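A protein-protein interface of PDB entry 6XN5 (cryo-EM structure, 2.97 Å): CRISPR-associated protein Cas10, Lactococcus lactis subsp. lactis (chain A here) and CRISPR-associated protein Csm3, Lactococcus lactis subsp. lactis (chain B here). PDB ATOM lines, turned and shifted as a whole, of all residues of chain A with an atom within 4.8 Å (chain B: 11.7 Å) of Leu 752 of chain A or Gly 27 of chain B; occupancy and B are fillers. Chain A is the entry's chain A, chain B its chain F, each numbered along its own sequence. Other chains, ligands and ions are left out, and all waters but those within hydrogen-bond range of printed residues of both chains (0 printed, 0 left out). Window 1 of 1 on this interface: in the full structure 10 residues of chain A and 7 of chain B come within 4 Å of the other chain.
The backbone carbonyl oxygen of Val 29 of chain B lies close to the side-chain amide nitrogen of Gln 134 of chain B. The backbone NH of Ile 511 of chain A is in hydrogen-bond range of the backbone carbonyl oxygen of Leu 752 of chain A (3.1 Å).
The backbone carbonyl oxygen (O) of Ile 26 of chain B is in hydrogen-bond range of the guanidinium group (NH2) of Arg 755 of chain A (2.8 Å). The backbone carbonyl oxygen (O) of Gly 27 of chain B lies within hydrogen-bond range of the guanidinium group (NH2) of Arg 755 of chain A (2.9 Å). The guanidinium group (NH2) of Arg 755 of chain A lies within hydrogen-bond range of the backbone carbonyl oxygen (O) of Ala 28 of chain B (3.4 Å).
Hydrophobic or aromatic side chains of chain A within 4 Å of the printed part of chain B: Tyr 693, Ile 751 and Leu 752. Of the 18 printed residues of chain B, 4 touch a printed residue of chain A. Among the printed residues, no Asp or Glu carboxylate lies within 4 Å of a Lys or Arg side-chain nitrogen of the other chain.
Tyr 693 of chain A touches Gly 27 of chain B. CD2 of Tyr 693 of chain A touches CA of Ala 28 of chain B, 3.7 Å away. CG1 of Val 29 of chain B touches OH of Tyr 693 of chain A, 3.4 Å away. Ile 751 of chain A touches Gly 27 of chain B. Gly 27 of chain B touches Leu 752 of chain A. CG1 of Val 29 of chain B touches NH2 of Arg 755 of chain A, at 3.4 Å.
Leu 752 of chain A touches just one residue of chain B: Gly 27 (3.7 Å). Gly 27 of chain B touches just these residues of chain A: Tyr 693 (3.2 Å), Ile 751 (3.3 Å), Leu 752 (3.7 Å) and Arg 755 (2.9 Å). No residue of chain B comes within 4 Å of Gly 510 of chain A. No residue of chain B comes within 4 Å of Glu 748 of chain A. Lys 753 of chain A touches none of the printed residues of chain B. No residue of chain B comes within 4 Å of Thr 754 of chain A. Printed residues of chain A within 4 Å of Val 29 of chain B: Tyr 693 and Arg 755. Of the printed residues of chain B, Tyr 693 of chain A touches Gly 27 (3.2 Å), Ala 28 (3.7 Å) and Val 29 (3.4 Å). Of the printed residues of chain A, Ile 26 of chain B touches Arg 755 (2.8 Å). Of the printed residues of chain A, Ala 28 of chain B touches Tyr 693 (3.7 Å) and Arg 755 (3.4 Å). Ile 749 of chain A touches none of the printed residues of chain B. The nearest printed residue of chain A that does not touch Gly 27 of chain B is Glu 748 of chain A (5.8 Å).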
ATOM      1  N   GLY A 510     -31.835  -1.462 -23.156  1.00  0.00           N
ATOM      2  CA  GLY A 510     -31.006  -0.347 -22.754  1.00  0.00           C
ATOM      3  C   GLY A 510     -31.055   0.813 -23.727  1.00  0.00           C
ATOM      4  O   GLY A 510     -31.888   0.880 -24.627  1.00  0.00           O
ATOM      5  N   ILE A 511     -30.133   1.755 -23.516  1.00  0.00           N
ATOM      6  CA  ILE A 511     -29.975   2.868 -24.440  1.00  0.00           C
ATOM      7  C   ILE A 511     -29.379   2.345 -25.744  1.00  0.00           C
ATOM      8  O   ILE A 511     -28.720   1.298 -25.774  1.00  0.00           O
ATOM      9  CB  ILE A 511     -29.116   3.965 -23.785  1.00  0.00           C
ATOM     10  CG1 ILE A 511     -29.264   5.307 -24.501  1.00  0.00           C
ATOM     11  CG2 ILE A 511     -27.672   3.555 -23.718  1.00  0.00           C
ATOM     12  CD1 ILE A 511     -28.466   6.424 -23.875  1.00  0.00           C
ATOM     13  N   TRP A 584     -23.228  -1.939 -25.866  1.00  0.00           N
ATOM     14  CA  TRP A 584     -22.465  -1.510 -24.698  1.00  0.00           C
ATOM     15  C   TRP A 584     -22.774  -2.365 -23.479  1.00  0.00           C
ATOM     16  O   TRP A 584     -21.916  -2.528 -22.601  1.00  0.00           O
ATOM     17  CB  TRP A 584     -22.742  -0.034 -24.412  1.00  0.00           C
ATOM     18  CG  TRP A 584     -24.031   0.202 -23.750  1.00  0.00           C
ATOM     19  CD1 TRP A 584     -25.247   0.297 -24.340  1.00  0.00           C
ATOM     20  CD2 TRP A 584     -24.248   0.359 -22.349  1.00  0.00           C
ATOM     21  NE1 TRP A 584     -26.214   0.504 -23.393  1.00  0.00           N
ATOM     22  CE2 TRP A 584     -25.623   0.545 -22.159  1.00  0.00           C
ATOM     23  CE3 TRP A 584     -23.408   0.350 -21.235  1.00  0.00           C
ATOM     24  CZ2 TRP A 584     -26.179   0.730 -20.905  1.00  0.00           C
ATOM     25  CZ3 TRP A 584     -23.958   0.533 -19.993  1.00  0.00           C
ATOM     26  CH2 TRP A 584     -25.330   0.719 -19.836  1.00  0.00           C
ATOM     27  N   GLN A 585     -23.980  -2.929 -23.418  1.00  0.00           N
ATOM     28  CA  GLN A 585     -24.319  -3.851 -22.345  1.00  0.00           C
ATOM     29  C   GLN A 585     -23.493  -5.124 -22.440  1.00  0.00           C
ATOM     30  O   GLN A 585     -23.024  -5.647 -21.424  1.00  0.00           O
ATOM     31  CB  GLN A 585     -25.809  -4.169 -22.399  1.00  0.00           C
ATOM     32  CG  GLN A 585     -26.685  -2.944 -22.290  1.00  0.00           C
ATOM     33  CD  GLN A 585     -28.106  -3.286 -21.927  1.00  0.00           C
ATOM     34  OE1 GLN A 585     -28.804  -2.496 -21.298  1.00  0.00           O
ATOM     35  NE2 GLN A 585     -28.544  -4.476 -22.311  1.00  0.00           N
ATOM     36  N   MET A 614     -18.849   4.632 -24.408  1.00  0.00           N
ATOM     37  CA  MET A 614     -20.147   4.475 -25.046  1.00  0.00           C
ATOM     38  C   MET A 614     -20.439   5.653 -25.968  1.00  0.00           C
ATOM     39  O   MET A 614     -20.180   6.812 -25.630  1.00  0.00           O
ATOM     40  CB  MET A 614     -21.251   4.276 -24.005  1.00  0.00           C
ATOM     41  CG  MET A 614     -21.528   5.429 -23.068  1.00  0.00           C
ATOM     42  SD  MET A 614     -22.853   5.007 -21.939  1.00  0.00           S
ATOM     43  CE  MET A 614     -24.230   5.057 -23.061  1.00  0.00           C
ATOM     44  N   TYR A 693     -33.985   9.166 -10.658  1.00  0.00           N
ATOM     45  CA  TYR A 693     -33.195  10.209 -11.316  1.00  0.00           C
ATOM     46  C   TYR A 693     -32.983  11.419 -10.413  1.00  0.00           C
ATOM     47  O   TYR A 693     -31.919  12.048 -10.465  1.00  0.00           O
ATOM     48  CB  TYR A 693     -33.822  10.643 -12.647  1.00  0.00           C
ATOM     49  CG  TYR A 693     -33.768   9.642 -13.789  1.00  0.00           C
ATOM     50  CD1 TYR A 693     -34.439   8.433 -13.743  1.00  0.00           C
ATOM     51  CD2 TYR A 693     -33.037   9.931 -14.928  1.00  0.00           C
ATOM     52  CE1 TYR A 693     -34.387   7.536 -14.786  1.00  0.00           C
ATOM     53  CE2 TYR A 693     -32.975   9.043 -15.977  1.00  0.00           C
ATOM     54  CZ  TYR A 693     -33.651   7.847 -15.904  1.00  0.00           C
ATOM     55  OH  TYR A 693     -33.589   6.960 -16.953  1.00  0.00           O
ATOM     56  N   GLU A 748     -26.177   4.773 -12.227  1.00  0.00           N
ATOM     57  CA  GLU A 748     -26.025   5.286 -13.583  1.00  0.00           C
ATOM     58  C   GLU A 748     -26.136   4.170 -14.610  1.00  0.00           C
ATOM     59  O   GLU A 748     -26.857   4.305 -15.601  1.00  0.00           O
ATOM     60  CB  GLU A 748     -24.689   6.013 -13.721  1.00  0.00           C
ATOM     61  CG  GLU A 748     -24.752   7.482 -13.360  1.00  0.00           C
ATOM     62  CD  GLU A 748     -23.389   8.142 -13.354  1.00  0.00           C
ATOM     63  OE1 GLU A 748     -22.382   7.431 -13.550  1.00  0.00           O
ATOM     64  OE2 GLU A 748     -23.320   9.371 -13.154  1.00  0.00           O
ATOM     65  N   ILE A 749     -25.469   3.038 -14.371  1.00  0.00           N
ATOM     66  CA  ILE A 749     -25.583   1.963 -15.349  1.00  0.00           C
ATOM     67  C   ILE A 749     -26.952   1.300 -15.279  1.00  0.00           C
ATOM     68  O   ILE A 749     -27.418   0.756 -16.280  1.00  0.00           O
ATOM     69  CB  ILE A 749     -24.451   0.928 -15.217  1.00  0.00           C
ATOM     70  CG1 ILE A 749     -24.470   0.236 -13.865  1.00  0.00           C
ATOM     71  CG2 ILE A 749     -23.119   1.570 -15.446  1.00  0.00           C
ATOM     72  CD1 ILE A 749     -23.532  -0.933 -13.787  1.00  0.00           C
ATOM     73  N   TYR A 750     -27.650   1.384 -14.139  1.00  0.00           N
ATOM     74  CA  TYR A 750     -29.019   0.869 -14.081  1.00  0.00           C
ATOM     75  C   TYR A 750     -29.967   1.710 -14.931  1.00  0.00           C
ATOM     76  O   TYR A 750     -30.753   1.174 -15.722  1.00  0.00           O
ATOM     77  CB  TYR A 750     -29.516   0.819 -12.637  1.00  0.00           C
ATOM     78  CG  TYR A 750     -31.008   0.596 -12.545  1.00  0.00           C
ATOM     79  CD1 TYR A 750     -31.562  -0.631 -12.879  1.00  0.00           C
ATOM     80  CD2 TYR A 750     -31.863   1.613 -12.135  1.00  0.00           C
ATOM     81  CE1 TYR A 750     -32.923  -0.843 -12.807  1.00  0.00           C
ATOM     82  CE2 TYR A 750     -33.225   1.411 -12.066  1.00  0.00           C
ATOM     83  CZ  TYR A 750     -33.746   0.180 -12.401  1.00  0.00           C
ATOM     84  OH  TYR A 750     -35.101  -0.028 -12.330  1.00  0.00           O
ATOM     85  N   ILE A 751     -29.902   3.033 -14.784  1.00  0.00           N
ATOM     86  CA  ILE A 751     -30.791   3.893 -15.558  1.00  0.00           C
ATOM     87  C   ILE A 751     -30.351   3.999 -17.010  1.00  0.00           C
ATOM     88  O   ILE A 751     -31.130   4.428 -17.868  1.00  0.00           O
ATOM     89  CB  ILE A 751     -30.909   5.268 -14.881  1.00  0.00           C
ATOM     90  CG1 ILE A 751     -29.617   6.068 -15.047  1.00  0.00           C
ATOM     91  CG2 ILE A 751     -31.340   5.109 -13.439  1.00  0.00           C
ATOM     92  CD1 ILE A 751     -29.814   7.548 -15.026  1.00  0.00           C
ATOM     93  N   LEU A 752     -29.107   3.625 -17.318  1.00  0.00           N
ATOM     94  CA  LEU A 752     -28.717   3.484 -18.716  1.00  0.00           C
ATOM     95  C   LEU A 752     -29.199   2.159 -19.294  1.00  0.00           C
ATOM     96  O   LEU A 752     -29.575   2.091 -20.468  1.00  0.00           O
ATOM     97  CB  LEU A 752     -27.202   3.622 -18.858  1.00  0.00           C
ATOM     98  CG  LEU A 752     -26.603   4.989 -19.215  1.00  0.00           C
ATOM     99  CD1 LEU A 752     -27.015   5.375 -20.596  1.00  0.00           C
ATOM    100  CD2 LEU A 752     -27.009   6.081 -18.275  1.00  0.00           C
ATOM    101  N   LYS A 753     -29.203   1.095 -18.485  1.00  0.00           N
ATOM    102  CA  LYS A 753     -29.720  -0.191 -18.933  1.00  0.00           C
ATOM    103  C   LYS A 753     -31.235  -0.204 -19.031  1.00  0.00           C
ATOM    104  O   LYS A 753     -31.793  -1.106 -19.661  1.00  0.00           O
ATOM    105  CB  LYS A 753     -29.273  -1.307 -17.986  1.00  0.00           C
ATOM    106  CG  LYS A 753     -27.867  -1.826 -18.213  1.00  0.00           C
ATOM    107  CD  LYS A 753     -27.452  -2.777 -17.108  1.00  0.00           C
ATOM    108  CE  LYS A 753     -28.134  -4.123 -17.255  1.00  0.00           C
ATOM    109  NZ  LYS A 753     -27.686  -4.844 -18.478  1.00  0.00           N
ATOM    110  N   THR A 754     -31.914   0.746 -18.399  1.00  0.00           N
ATOM    111  CA  THR A 754     -33.371   0.810 -18.422  1.00  0.00           C
ATOM    112  C   THR A 754     -33.795   2.117 -19.089  1.00  0.00           C
ATOM    113  O   THR A 754     -33.899   3.159 -18.442  1.00  0.00           O
ATOM    114  CB  THR A 754     -33.939   0.694 -17.016  1.00  0.00           C
ATOM    115  OG1 THR A 754     -33.341   1.690 -16.178  1.00  0.00           O
ATOM    116  CG2 THR A 754     -33.651  -0.685 -16.444  1.00  0.00           C
ATOM    117  N   ARG A 755     -34.041   2.051 -20.395  1.00  0.00           N
ATOM    118  CA  ARG A 755     -34.578   3.170 -21.155  1.00  0.00           C
ATOM    119  C   ARG A 755     -35.468   2.629 -22.265  1.00  0.00           C
ATOM    120  O   ARG A 755     -35.798   1.441 -22.305  1.00  0.00           O
ATOM    121  CB  ARG A 755     -33.471   4.048 -21.745  1.00  0.00           C
ATOM    122  CG  ARG A 755     -33.050   5.217 -20.882  1.00  0.00           C
ATOM    123  CD  ARG A 755     -31.815   5.855 -21.474  1.00  0.00           C
ATOM    124  NE  ARG A 755     -31.367   7.042 -20.756  1.00  0.00           N
ATOM    125  CZ  ARG A 755     -31.448   8.276 -21.240  1.00  0.00           C
ATOM    126  NH1 ARG A 755     -31.963   8.486 -22.443  1.00  0.00           N
ATOM    127  NH2 ARG A 755     -31.011   9.301 -20.523  1.00  0.00           N
ATOM    128  N   SER B  20     -24.796  17.823 -26.727  1.00  0.00           N
ATOM    129  CA  SER B  20     -23.532  17.122 -26.658  1.00  0.00           C
ATOM    130  C   SER B  20     -23.772  15.647 -26.366  1.00  0.00           C
ATOM    131  O   SER B  20     -24.709  15.268 -25.659  1.00  0.00           O
ATOM    132  CB  SER B  20     -22.636  17.739 -25.585  1.00  0.00           C
ATOM    133  OG  SER B  20     -22.400  19.110 -25.850  1.00  0.00           O
ATOM    134  N   SER B  21     -22.915  14.810 -26.935  1.00  0.00           N
ATOM    135  CA  SER B  21     -22.929  13.371 -26.712  1.00  0.00           C
ATOM    136  C   SER B  21     -21.613  12.935 -26.091  1.00  0.00           C
ATOM    137  O   SER B  21     -21.065  11.875 -26.406  1.00  0.00           O
ATOM    138  CB  SER B  21     -23.202  12.622 -28.014  1.00  0.00           C
ATOM    139  OG  SER B  21     -24.515  12.878 -28.478  1.00  0.00           O
ATOM    140  N   ASP B  22     -21.097  13.759 -25.184  1.00  0.00           N
ATOM    141  CA  ASP B  22     -19.768  13.608 -24.615  1.00  0.00           C
ATOM    142  C   ASP B  22     -19.759  12.835 -23.303  1.00  0.00           C
ATOM    143  O   ASP B  22     -18.714  12.782 -22.640  1.00  0.00           O
ATOM    144  CB  ASP B  22     -19.138  14.992 -24.435  1.00  0.00           C
ATOM    145  CG  ASP B  22     -20.033  15.950 -23.659  1.00  0.00           C
ATOM    146  OD1 ASP B  22     -21.180  15.580 -23.333  1.00  0.00           O
ATOM    147  OD2 ASP B  22     -19.591  17.087 -23.392  1.00  0.00           O
ATOM    148  N   PHE B  23     -20.896  12.224 -22.942  1.00  0.00           N
ATOM    149  CA  PHE B  23     -21.121  11.516 -21.677  1.00  0.00           C
ATOM    150  C   PHE B  23     -20.825  12.474 -20.512  1.00  0.00           C
ATOM    151  O   PHE B  23     -20.127  12.164 -19.550  1.00  0.00           O
ATOM    152  CB  PHE B  23     -20.314  10.196 -21.640  1.00  0.00           C
ATOM    153  CG  PHE B  23     -20.528   9.330 -20.405  1.00  0.00           C
ATOM    154  CD1 PHE B  23     -21.693   8.589 -20.276  1.00  0.00           C
ATOM    155  CD2 PHE B  23     -19.544   9.183 -19.436  1.00  0.00           C
ATOM    156  CE1 PHE B  23     -21.902   7.779 -19.176  1.00  0.00           C
ATOM    157  CE2 PHE B  23     -19.757   8.392 -18.324  1.00  0.00           C
ATOM    158  CZ  PHE B  23     -20.932   7.678 -18.202  1.00  0.00           C
ATOM    159  N   SER B  24     -21.308  13.709 -20.642  1.00  0.00           N
ATOM    160  CA  SER B  24     -21.187  14.656 -19.541  1.00  0.00           C
ATOM    161  C   SER B  24     -22.224  14.347 -18.473  1.00  0.00           C
ATOM    162  O   SER B  24     -21.886  13.999 -17.336  1.00  0.00           O
ATOM    163  CB  SER B  24     -21.344  16.086 -20.059  1.00  0.00           C
ATOM    164  OG  SER B  24     -22.511  16.211 -20.849  1.00  0.00           O
ATOM    165  N   ALA B  25     -23.500  14.462 -18.835  1.00  0.00           N
ATOM    166  CA  ALA B  25     -24.571  13.815 -18.090  1.00  0.00           C
ATOM    167  C   ALA B  25     -25.637  13.458 -19.123  1.00  0.00           C
ATOM    168  O   ALA B  25     -26.509  14.278 -19.422  1.00  0.00           O
ATOM    169  CB  ALA B  25     -25.125  14.712 -16.996  1.00  0.00           C
ATOM    170  N   ILE B  26     -25.542  12.249 -19.671  1.00  0.00           N
ATOM    171  CA  ILE B  26     -26.588  11.691 -20.515  1.00  0.00           C
ATOM    172  C   ILE B  26     -27.412  10.665 -19.775  1.00  0.00           C
ATOM    173  O   ILE B  26     -28.287  10.027 -20.382  1.00  0.00           O
ATOM    174  CB  ILE B  26     -26.011  11.081 -21.804  1.00  0.00           C
ATOM    175  CG1 ILE B  26     -24.863  10.128 -21.467  1.00  0.00           C
ATOM    176  CG2 ILE B  26     -25.582  12.183 -22.765  1.00  0.00           C
ATOM    177  CD1 ILE B  26     -24.584   9.099 -22.540  1.00  0.00           C
ATOM    178  N   GLY B  27     -27.139  10.461 -18.486  1.00  0.00           N
ATOM    179  CA  GLY B  27     -27.962   9.564 -17.698  1.00  0.00           C
ATOM    180  C   GLY B  27     -29.371  10.084 -17.522  1.00  0.00           C
ATOM    181  O   GLY B  27     -30.342   9.349 -17.703  1.00  0.00           O
ATOM    182  N   ALA B  28     -29.496  11.370 -17.196  1.00  0.00           N
ATOM    183  CA  ALA B  28     -30.800  11.977 -16.979  1.00  0.00           C
ATOM    184  C   ALA B  28     -31.563  12.050 -18.290  1.00  0.00           C
ATOM    185  O   ALA B  28     -31.007  12.449 -19.318  1.00  0.00           O
ATOM    186  CB  ALA B  28     -30.635  13.371 -16.377  1.00  0.00           C
ATOM    187  N   VAL B  29     -32.840  11.670 -18.256  1.00  0.00           N
ATOM    188  CA  VAL B  29     -33.638  11.693 -19.473  1.00  0.00           C
ATOM    189  C   VAL B  29     -34.061  13.130 -19.764  1.00  0.00           C
ATOM    190  O   VAL B  29     -35.172  13.571 -19.461  1.00  0.00           O
ATOM    191  CB  VAL B  29     -34.798  10.670 -19.403  1.00  0.00           C
ATOM    192  CG1 VAL B  29     -34.231   9.288 -19.314  1.00  0.00           C
ATOM    193  CG2 VAL B  29     -35.612  10.795 -18.102  1.00  0.00           C
ATOM    194  N   ALA B  30     -33.156  13.854 -20.412  1.00  0.00           N
ATOM    195  CA  ALA B  30     -33.328  15.253 -20.764  1.00  0.00           C
ATOM    196  C   ALA B  30     -32.322  15.574 -21.854  1.00  0.00           C
ATOM    197  O   ALA B  30     -31.129  15.306 -21.693  1.00  0.00           O
ATOM    198  CB  ALA B  30     -33.118  16.164 -19.556  1.00  0.00           C
ATOM    199  N   SER B  31     -32.790  16.112 -22.967  1.00  0.00           N
ATOM    200  CA  SER B  31     -31.902  16.456 -24.059  1.00  0.00           C
ATOM    201  C   SER B  31     -31.091  17.676 -23.665  1.00  0.00           C
ATOM    202  O   SER B  31     -31.681  18.717 -23.359  1.00  0.00           O
ATOM    203  CB  SER B  31     -32.703  16.740 -25.315  1.00  0.00           C
ATOM    204  OG  SER B  31     -33.686  17.722 -25.051  1.00  0.00           O
ATOM    205  N   PRO B  32     -29.767  17.603 -23.651  1.00  0.00           N
ATOM    206  CA  PRO B  32     -28.966  18.709 -23.126  1.00  0.00           C
ATOM    207  C   PRO B  32     -28.688  19.763 -24.187  1.00  0.00           C
ATOM    208  O   PRO B  32     -28.891  19.560 -25.381  1.00  0.00           O
ATOM    209  CB  PRO B  32     -27.680  18.015 -22.684  1.00  0.00           C
ATOM    210  CG  PRO B  32     -27.548  16.876 -23.630  1.00  0.00           C
ATOM    211  CD  PRO B  32     -28.929  16.468 -24.067  1.00  0.00           C
ATOM    212  N   ARG B  35     -22.722  23.386 -24.411  1.00  0.00           N
ATOM    213  CA  ARG B  35     -21.995  24.124 -23.395  1.00  0.00           C
ATOM    214  C   ARG B  35     -20.528  24.167 -23.784  1.00  0.00           C
ATOM    215  O   ARG B  35     -20.056  23.357 -24.585  1.00  0.00           O
ATOM    216  CB  ARG B  35     -22.134  23.491 -22.004  1.00  0.00           C
ATOM    217  CG  ARG B  35     -23.439  22.774 -21.739  1.00  0.00           C
ATOM    218  CD  ARG B  35     -23.375  21.961 -20.478  1.00  0.00           C
ATOM    219  NE  ARG B  35     -23.807  22.745 -19.333  1.00  0.00           N
ATOM    220  CZ  ARG B  35     -25.015  22.668 -18.792  1.00  0.00           C
ATOM    221  NH1 ARG B  35     -25.914  21.836 -19.296  1.00  0.00           N
ATOM    222  NH2 ARG B  35     -25.321  23.422 -17.748  1.00  0.00           N
ATOM    223  N   ARG B  40     -18.288  24.460 -18.774  1.00  0.00           N
ATOM    224  CA  ARG B  40     -19.625  23.846 -18.747  1.00  0.00           C
ATOM    225  C   ARG B  40     -20.729  24.881 -18.554  1.00  0.00           C
ATOM    226  O   ARG B  40     -21.744  24.621 -17.909  1.00  0.00           O
ATOM    227  CB  ARG B  40     -19.715  22.733 -17.706  1.00  0.00           C
ATOM    228  CG  ARG B  40     -18.850  21.540 -18.042  1.00  0.00           C
ATOM    229  CD  ARG B  40     -19.573  20.611 -18.990  1.00  0.00           C
ATOM    230  NE  ARG B  40     -19.074  20.720 -20.355  1.00  0.00           N
ATOM    231  CZ  ARG B  40     -19.558  20.030 -21.383  1.00  0.00           C
ATOM    232  NH1 ARG B  40     -20.557  19.180 -21.197  1.00  0.00           N
ATOM    233  NH2 ARG B  40     -19.045  20.187 -22.594  1.00  0.00           N
ATOM    234  N   VAL B 117     -34.829  22.919 -16.813  1.00  0.00           N
ATOM    235  CA  VAL B 117     -35.387  21.774 -17.515  1.00  0.00           C
ATOM    236  C   VAL B 117     -36.874  22.031 -17.715  1.00  0.00           C
ATOM    237  O   VAL B 117     -37.549  22.577 -16.836  1.00  0.00           O
ATOM    238  CB  VAL B 117     -35.084  20.450 -16.771  1.00  0.00           C
ATOM    239  CG1 VAL B 117     -35.689  20.419 -15.372  1.00  0.00           C
ATOM    240  CG2 VAL B 117     -35.530  19.246 -17.582  1.00  0.00           C
ATOM    241  N   GLN B 134     -38.255  15.522 -21.393  1.00  0.00           N
ATOM    242  CA  GLN B 134     -37.608  16.684 -20.810  1.00  0.00           C
ATOM    243  C   GLN B 134     -36.666  17.335 -21.805  1.00  0.00           C
ATOM    244  O   GLN B 134     -36.071  16.685 -22.664  1.00  0.00           O
ATOM    245  CB  GLN B 134     -36.834  16.322 -19.555  1.00  0.00           C
ATOM    246  CG  GLN B 134     -37.681  16.124 -18.356  1.00  0.00           C
ATOM    247  CD  GLN B 134     -37.133  15.074 -17.431  1.00  0.00           C
ATOM    248  OE1 GLN B 134     -36.215  15.332 -16.657  1.00  0.00           O
ATOM    249  NE2 GLN B 134     -37.691  13.873 -17.506  1.00  0.00           N
ATOM    250  N   GLU B 136     -33.585  20.313 -21.712  1.00  0.00           N
ATOM    251  CA  GLU B 136     -32.775  21.366 -21.125  1.00  0.00           C
ATOM    252  C   GLU B 136     -32.965  22.644 -21.923  1.00  0.00           C
ATOM    253  O   GLU B 136     -32.983  22.624 -23.154  1.00  0.00           O
ATOM    254  CB  GLU B 136     -31.299  20.984 -21.108  1.00  0.00           C
ATOM    255  CG  GLU B 136     -30.838  20.212 -19.902  1.00  0.00           C
ATOM    256  CD  GLU B 136     -30.549  21.124 -18.739  1.00  0.00           C
ATOM    257  OE1 GLU B 136     -30.145  22.273 -19.001  1.00  0.00           O
ATOM    258  OE2 GLU B 136     -30.707  20.701 -17.574  1.00  0.00           O
